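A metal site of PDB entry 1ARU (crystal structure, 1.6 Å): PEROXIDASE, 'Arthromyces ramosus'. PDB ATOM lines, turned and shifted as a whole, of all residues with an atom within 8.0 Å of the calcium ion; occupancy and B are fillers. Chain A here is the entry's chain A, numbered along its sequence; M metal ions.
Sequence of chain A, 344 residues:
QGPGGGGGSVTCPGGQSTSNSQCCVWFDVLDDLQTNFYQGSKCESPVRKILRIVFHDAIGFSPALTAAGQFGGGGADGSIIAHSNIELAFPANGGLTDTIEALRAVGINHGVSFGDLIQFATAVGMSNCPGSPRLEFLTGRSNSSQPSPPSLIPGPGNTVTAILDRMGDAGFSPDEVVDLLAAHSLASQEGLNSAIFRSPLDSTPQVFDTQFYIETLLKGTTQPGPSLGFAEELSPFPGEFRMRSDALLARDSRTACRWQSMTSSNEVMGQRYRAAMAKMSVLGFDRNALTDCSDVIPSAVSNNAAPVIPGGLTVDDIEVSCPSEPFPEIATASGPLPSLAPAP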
ATOM      1  N   PRO A 130       3.105  -4.298 -15.222  1.00  0.00           N
ATOM      2  CA  PRO A 130       3.714  -3.693 -16.409  1.00  0.00           C
ATOM      3  C   PRO A 130       4.546  -4.674 -17.226  1.00  0.00           C
ATOM      4  O   PRO A 130       5.312  -5.469 -16.666  1.00  0.00           O
ATOM      5  CB  PRO A 130       4.531  -2.547 -15.880  1.00  0.00           C
ATOM      6  CG  PRO A 130       3.810  -2.162 -14.598  1.00  0.00           C
ATOM      7  CD  PRO A 130       3.370  -3.497 -14.025  1.00  0.00           C
ATOM      8  N   ALA A 182       8.960 -17.898 -17.189  1.00  0.00           N
ATOM      9  CA  ALA A 182       8.973 -16.445 -17.228  1.00  0.00           C
ATOM     10  C   ALA A 182       8.136 -15.903 -16.070  1.00  0.00           C
ATOM     11  O   ALA A 182       8.340 -14.764 -15.609  1.00  0.00           O
ATOM     12  CB  ALA A 182       8.393 -15.905 -18.533  1.00  0.00           C
ATOM     13  N   ALA A 183       7.218 -16.703 -15.518  1.00  0.00           N
ATOM     14  CA  ALA A 183       6.441 -16.253 -14.373  1.00  0.00           C
ATOM     15  C   ALA A 183       7.313 -15.958 -13.165  1.00  0.00           C
ATOM     16  O   ALA A 183       6.916 -15.170 -12.318  1.00  0.00           O
ATOM     17  CB  ALA A 183       5.433 -17.286 -13.963  1.00  0.00           C
ATOM     18  N   HIS A 184       8.542 -16.496 -13.037  1.00  0.00           N
ATOM     19  CA  HIS A 184       9.390 -16.147 -11.904  1.00  0.00           C
ATOM     20  C   HIS A 184       9.973 -14.731 -12.015  1.00  0.00           C
ATOM     21  O   HIS A 184      10.771 -14.282 -11.171  1.00  0.00           O
ATOM     22  CB  HIS A 184      10.512 -17.189 -11.744  1.00  0.00           C
ATOM     23  CG  HIS A 184      10.103 -18.474 -11.038  1.00  0.00           C
ATOM     24  ND1 HIS A 184      11.001 -19.445 -10.590  1.00  0.00           N
ATOM     25  CD2 HIS A 184       8.806 -18.866 -10.718  1.00  0.00           C
ATOM     26  CE1 HIS A 184      10.272 -20.390 -10.001  1.00  0.00           C
ATOM     27  NE2 HIS A 184       9.018 -20.086 -10.062  1.00  0.00           N
ATOM     28  N   SER A 185       9.620 -14.013 -13.077  1.00  0.00           N
ATOM     29  CA  SER A 185      10.001 -12.617 -13.224  1.00  0.00           C
ATOM     30  C   SER A 185       9.030 -11.839 -12.338  1.00  0.00           C
ATOM     31  O   SER A 185       9.250 -10.648 -12.156  1.00  0.00           O
ATOM     32  CB  SER A 185       9.844 -12.140 -14.667  1.00  0.00           C
ATOM     33  OG  SER A 185      10.281 -10.783 -14.859  1.00  0.00           O
ATOM     34  N   LEU A 186       7.983 -12.400 -11.747  1.00  0.00           N
ATOM     35  CA  LEU A 186       7.039 -11.671 -10.908  1.00  0.00           C
ATOM     36  C   LEU A 186       6.950 -12.574  -9.680  1.00  0.00           C
ATOM     37  O   LEU A 186       5.899 -13.120  -9.340  1.00  0.00           O
ATOM     38  CB  LEU A 186       5.754 -11.601 -11.719  1.00  0.00           C
ATOM     39  CG  LEU A 186       5.107 -10.368 -12.341  1.00  0.00           C
ATOM     40  CD1 LEU A 186       6.073  -9.244 -12.673  1.00  0.00           C
ATOM     41  CD2 LEU A 186       4.337 -10.893 -13.527  1.00  0.00           C
ATOM     42  N   ALA A 187       8.061 -12.747  -8.967  1.00  0.00           N
ATOM     43  CA  ALA A 187       8.092 -13.742  -7.906  1.00  0.00           C
ATOM     44  C   ALA A 187       8.935 -13.456  -6.699  1.00  0.00           C
ATOM     45  O   ALA A 187       9.904 -12.687  -6.752  1.00  0.00           O
ATOM     46  CB  ALA A 187       8.578 -15.065  -8.463  1.00  0.00           C
ATOM     47  N   PRO A 200      12.689 -11.219  -3.472  1.00  0.00           N
ATOM     48  CA  PRO A 200      12.376 -11.429  -4.876  1.00  0.00           C
ATOM     49  C   PRO A 200      13.308 -12.409  -5.587  1.00  0.00           C
ATOM     50  O   PRO A 200      14.465 -12.583  -5.186  1.00  0.00           O
ATOM     51  CB  PRO A 200      12.427 -10.046  -5.510  1.00  0.00           C
ATOM     52  CG  PRO A 200      12.432  -9.076  -4.358  1.00  0.00           C
ATOM     53  CD  PRO A 200      13.138  -9.856  -3.258  1.00  0.00           C
ATOM     54  N   LEU A 201      12.819 -13.008  -6.687  1.00  0.00           N
ATOM     55  CA  LEU A 201      13.602 -13.897  -7.513  1.00  0.00           C
ATOM     56  C   LEU A 201      14.263 -13.067  -8.609  1.00  0.00           C
ATOM     57  O   LEU A 201      15.147 -13.592  -9.289  1.00  0.00           O
ATOM     58  CB  LEU A 201      12.690 -14.970  -8.060  1.00  0.00           C
ATOM     59  CG  LEU A 201      12.669 -16.327  -7.328  1.00  0.00           C
ATOM     60  CD1 LEU A 201      12.667 -16.166  -5.812  1.00  0.00           C
ATOM     61  CD2 LEU A 201      11.470 -17.121  -7.839  1.00  0.00           C
ATOM     62  N   ASP A 202      13.827 -11.847  -8.935  1.00  0.00           N
ATOM     63  CA  ASP A 202      14.626 -11.020  -9.818  1.00  0.00           C
ATOM     64  C   ASP A 202      14.525  -9.587  -9.274  1.00  0.00           C
ATOM     65  O   ASP A 202      13.728  -9.341  -8.367  1.00  0.00           O
ATOM     66  CB  ASP A 202      14.159 -11.124 -11.312  1.00  0.00           C
ATOM     67  CG  ASP A 202      12.933 -10.373 -11.821  1.00  0.00           C
ATOM     68  OD1 ASP A 202      12.250  -9.658 -11.092  1.00  0.00           O
ATOM     69  OD2 ASP A 202      12.642 -10.517 -13.009  1.00  0.00           O
ATOM     70  N   SER A 203      15.226  -8.587  -9.844  1.00  0.00           N
ATOM     71  CA  SER A 203      15.196  -7.248  -9.285  1.00  0.00           C
ATOM     72  C   SER A 203      13.934  -6.442  -9.609  1.00  0.00           C
ATOM     73  O   SER A 203      13.861  -5.284  -9.189  1.00  0.00           O
ATOM     74  CB  SER A 203      16.429  -6.493  -9.759  1.00  0.00           C
ATOM     75  OG  SER A 203      16.469  -6.420 -11.183  1.00  0.00           O
ATOM     76  N   THR A 204      12.972  -6.946 -10.374  1.00  0.00           N
ATOM     77  CA  THR A 204      11.766  -6.219 -10.708  1.00  0.00           C
ATOM     78  C   THR A 204      10.579  -7.158 -10.470  1.00  0.00           C
ATOM     79  O   THR A 204       9.940  -7.630 -11.431  1.00  0.00           O
ATOM     80  CB  THR A 204      11.881  -5.771 -12.178  1.00  0.00           C
ATOM     81  OG1 THR A 204      12.199  -6.929 -12.935  1.00  0.00           O
ATOM     82  CG2 THR A 204      12.965  -4.737 -12.416  1.00  0.00           C
ATOM     83  N   PRO A 205      10.225  -7.513  -9.222  1.00  0.00           N
ATOM     84  CA  PRO A 205       9.146  -8.430  -8.959  1.00  0.00           C
ATOM     85  C   PRO A 205       7.787  -7.907  -9.383  1.00  0.00           C
ATOM     86  O   PRO A 205       6.795  -8.635  -9.336  1.00  0.00           O
ATOM     87  CB  PRO A 205       9.253  -8.719  -7.475  1.00  0.00           C
ATOM     88  CG  PRO A 205       9.863  -7.449  -6.916  1.00  0.00           C
ATOM     89  CD  PRO A 205      10.882  -7.105  -7.978  1.00  0.00           C
ATOM     90  N   GLN A 206       7.718  -6.619  -9.724  1.00  0.00           N
ATOM     91  CA  GLN A 206       6.480  -6.037 -10.204  1.00  0.00           C
ATOM     92  C   GLN A 206       6.562  -5.715 -11.699  1.00  0.00           C
ATOM     93  O   GLN A 206       5.715  -4.940 -12.182  1.00  0.00           O
ATOM     94  CB  GLN A 206       6.157  -4.767  -9.408  1.00  0.00           C
ATOM     95  CG  GLN A 206       5.756  -5.066  -7.966  1.00  0.00           C
ATOM     96  CD  GLN A 206       5.210  -3.806  -7.276  1.00  0.00           C
ATOM     97  OE1 GLN A 206       5.943  -2.861  -6.991  1.00  0.00           O
ATOM     98  NE2 GLN A 206       3.934  -3.725  -6.943  1.00  0.00           N
ATOM     99  N   VAL A 207       7.527  -6.179 -12.504  1.00  0.00           N
ATOM    100  CA  VAL A 207       7.574  -5.889 -13.940  1.00  0.00           C
ATOM    101  C   VAL A 207       7.810  -7.224 -14.668  1.00  0.00           C
ATOM    102  O   VAL A 207       8.744  -7.959 -14.309  1.00  0.00           O
ATOM    103  CB  VAL A 207       8.745  -4.945 -14.329  1.00  0.00           C
ATOM    104  CG1 VAL A 207       8.712  -4.658 -15.829  1.00  0.00           C
ATOM    105  CG2 VAL A 207       8.627  -3.614 -13.619  1.00  0.00           C
ATOM    106  N   PHE A 208       6.964  -7.603 -15.627  1.00  0.00           N
ATOM    107  CA  PHE A 208       7.117  -8.838 -16.376  1.00  0.00           C
ATOM    108  C   PHE A 208       8.128  -8.531 -17.453  1.00  0.00           C
ATOM    109  O   PHE A 208       7.826  -7.916 -18.488  1.00  0.00           O
ATOM    110  CB  PHE A 208       5.794  -9.249 -16.984  1.00  0.00           C
ATOM    111  CG  PHE A 208       5.841 -10.588 -17.695  1.00  0.00           C
ATOM    112  CD1 PHE A 208       5.960 -11.756 -16.961  1.00  0.00           C
ATOM    113  CD2 PHE A 208       5.789 -10.627 -19.083  1.00  0.00           C
ATOM    114  CE1 PHE A 208       6.030 -12.972 -17.610  1.00  0.00           C
ATOM    115  CE2 PHE A 208       5.855 -11.833 -19.715  1.00  0.00           C
ATOM    116  CZ  PHE A 208       5.970 -12.988 -18.978  1.00  0.00           C
ATOM    117  N   ASP A 209       9.376  -8.916 -17.163  1.00  0.00           N
ATOM    118  CA  ASP A 209      10.521  -8.668 -18.017  1.00  0.00           C
ATOM    119  C   ASP A 209      11.529  -9.828 -18.002  1.00  0.00           C
ATOM    120  O   ASP A 209      11.452 -10.836 -17.281  1.00  0.00           O
ATOM    121  CB  ASP A 209      11.206  -7.356 -17.573  1.00  0.00           C
ATOM    122  CG  ASP A 209      11.660  -7.373 -16.104  1.00  0.00           C
ATOM    123  OD1 ASP A 209      11.684  -8.425 -15.453  1.00  0.00           O
ATOM    124  OD2 ASP A 209      12.012  -6.315 -15.606  1.00  0.00           O
ATOM    125  N   THR A 210      12.544  -9.647 -18.773  1.00  0.00           N
ATOM    126  CA  THR A 210      13.644 -10.571 -18.941  1.00  0.00           C
ATOM    127  C   THR A 210      14.638 -10.636 -17.747  1.00  0.00           C
ATOM    128  O   THR A 210      15.525 -11.505 -17.747  1.00  0.00           O
ATOM    129  CB  THR A 210      14.054  -9.945 -20.270  1.00  0.00           C
ATOM    130  OG1 THR A 210      13.630 -10.832 -21.309  1.00  0.00           O
ATOM    131  CG2 THR A 210      15.386  -9.395 -20.117  1.00  0.00           C
ATOM    132  N   GLN A 211      14.580  -9.747 -16.726  1.00  0.00           N
ATOM    133  CA  GLN A 211      15.571  -9.716 -15.664  1.00  0.00           C
ATOM    134  C   GLN A 211      15.776 -11.052 -14.974  1.00  0.00           C
ATOM    135  O   GLN A 211      16.925 -11.390 -14.665  1.00  0.00           O
ATOM    136  CB  GLN A 211      15.210  -8.669 -14.596  1.00  0.00           C
ATOM    137  CG  GLN A 211      15.329  -7.223 -15.073  1.00  0.00           C
ATOM    138  CD  GLN A 211      16.633  -6.866 -15.777  1.00  0.00           C
ATOM    139  OE1 GLN A 211      16.635  -6.339 -16.902  1.00  0.00           O
ATOM    140  NE2 GLN A 211      17.790  -7.073 -15.152  1.00  0.00           N
ATOM    141  N   PHE A 212      14.749 -11.859 -14.791  1.00  0.00           N
ATOM    142  CA  PHE A 212      14.895 -13.164 -14.159  1.00  0.00           C
ATOM    143  C   PHE A 212      15.869 -14.040 -14.900  1.00  0.00           C
ATOM    144  O   PHE A 212      16.731 -14.647 -14.266  1.00  0.00           O
ATOM    145  CB  PHE A 212      13.544 -13.853 -14.088  1.00  0.00           C
ATOM    146  CG  PHE A 212      13.622 -15.315 -13.698  1.00  0.00           C
ATOM    147  CD1 PHE A 212      13.967 -15.698 -12.412  1.00  0.00           C
ATOM    148  CD2 PHE A 212      13.361 -16.262 -14.673  1.00  0.00           C
ATOM    149  CE1 PHE A 212      14.043 -17.036 -12.111  1.00  0.00           C
ATOM    150  CE2 PHE A 212      13.440 -17.611 -14.353  1.00  0.00           C
ATOM    151  CZ  PHE A 212      13.780 -17.978 -13.079  1.00  0.00           C
ATOM    152  N   TYR A 213      15.806 -14.087 -16.238  1.00  0.00           N
ATOM    153  CA  TYR A 213      16.723 -14.944 -16.981  1.00  0.00           C
ATOM    154  C   TYR A 213      18.139 -14.422 -16.886  1.00  0.00           C
ATOM    155  O   TYR A 213      19.085 -15.198 -16.738  1.00  0.00           O
ATOM    156  CB  TYR A 213      16.260 -15.000 -18.444  1.00  0.00           C
ATOM    157  CG  TYR A 213      14.904 -15.712 -18.587  1.00  0.00           C
ATOM    158  CD1 TYR A 213      14.826 -17.092 -18.523  1.00  0.00           C
ATOM    159  CD2 TYR A 213      13.756 -14.982 -18.813  1.00  0.00           C
ATOM    160  CE1 TYR A 213      13.613 -17.754 -18.688  1.00  0.00           C
ATOM    161  CE2 TYR A 213      12.545 -15.649 -18.987  1.00  0.00           C
ATOM    162  CZ  TYR A 213      12.476 -17.027 -18.922  1.00  0.00           C
ATOM    163  OH  TYR A 213      11.267 -17.658 -19.153  1.00  0.00           O
ATOM    164  N   GLU A 215      19.541 -12.501 -14.399  1.00  0.00           N
ATOM    165  CA  GLU A 215      20.060 -12.578 -13.046  1.00  0.00           C
ATOM    166  C   GLU A 215      20.277 -13.969 -12.499  1.00  0.00           C
ATOM    167  O   GLU A 215      21.172 -14.103 -11.657  1.00  0.00           O
ATOM    168  CB  GLU A 215      19.116 -11.753 -12.157  1.00  0.00           C
ATOM    169  CG  GLU A 215      19.213 -10.254 -12.529  1.00  0.00           C
ATOM    170  CD  GLU A 215      18.180  -9.377 -11.874  1.00  0.00           C
ATOM    171  OE1 GLU A 215      17.582  -9.756 -10.871  1.00  0.00           O
ATOM    172  OE2 GLU A 215      17.938  -8.316 -12.403  1.00  0.00           O
ATOM    173  N   ASN A 266      12.105  -8.576 -24.392  1.00  0.00           N
ATOM    174  CA  ASN A 266      10.877  -8.678 -23.636  1.00  0.00           C
ATOM    175  C   ASN A 266       9.743  -9.114 -24.543  1.00  0.00           C
ATOM    176  O   ASN A 266       8.865  -9.892 -24.139  1.00  0.00           O
ATOM    177  CB  ASN A 266      10.513  -7.355 -23.002  1.00  0.00           C
ATOM    178  CG  ASN A 266      11.360  -7.051 -21.770  1.00  0.00           C
ATOM    179  OD1 ASN A 266      11.558  -7.888 -20.874  1.00  0.00           O
ATOM    180  ND2 ASN A 266      11.854  -5.822 -21.643  1.00  0.00           N
ATOM    181  N   MET A 269      10.079 -12.992 -25.146  1.00  0.00           N
ATOM    182  CA  MET A 269       9.739 -13.694 -23.921  1.00  0.00           C
ATOM    183  C   MET A 269       8.224 -13.700 -23.746  1.00  0.00           C
ATOM    184  O   MET A 269       7.653 -14.764 -23.525  1.00  0.00           O
ATOM    185  CB  MET A 269      10.351 -13.041 -22.683  1.00  0.00           C
ATOM    186  CG  MET A 269       9.851 -13.613 -21.347  1.00  0.00           C
ATOM    187  SD  MET A 269      10.493 -12.633 -19.968  1.00  0.00           S
ATOM    188  CE  MET A 269       9.311 -11.331 -20.123  1.00  0.00           C
ATOM    189  N   ASN A 303       6.056  -1.841 -20.708  1.00  0.00           N
ATOM    190  CA  ASN A 303       7.287  -1.660 -19.980  1.00  0.00           C
ATOM    191  C   ASN A 303       8.279  -1.002 -20.953  1.00  0.00           C
ATOM    192  O   ASN A 303       8.608  -1.504 -22.028  1.00  0.00           O
ATOM    193  CB  ASN A 303       7.801  -3.015 -19.518  1.00  0.00           C
ATOM    194  CG  ASN A 303       9.252  -2.952 -19.109  1.00  0.00           C
ATOM    195  OD1 ASN A 303       9.711  -1.934 -18.621  1.00  0.00           O
ATOM    196  ND2 ASN A 303      10.019  -4.020 -19.279  1.00  0.00           N
HETATM  197 CA    CA M   1      10.762  -9.013 -13.237  1.00  0.00          CA
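The nearest printed residue that does not touch the calcium ion is Pro 205 (4.3 Å).
The calcium ion is bound by OD2 of Asp 202 (2.4 Å), O of Thr 204 (2.4 Å), OG of Ser 185 (2.4 Å), OD1 of Asp 209 (2.5 Å), O of Ser 185 (2.5 Å), O of Val 207 (2.5 Å), OG1 of Thr 204 (2.5 Å) and OD1 of Asp 202 (2.7 Å).
The backbone NH (N) of Phe 212 lies close to the side-chain carboxylate (OD2) of Asp 202 (3.1 Å).
The backbone NH of Gln 211 lies close to the side-chain carboxylate of Asp 209 (3.4 Å).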
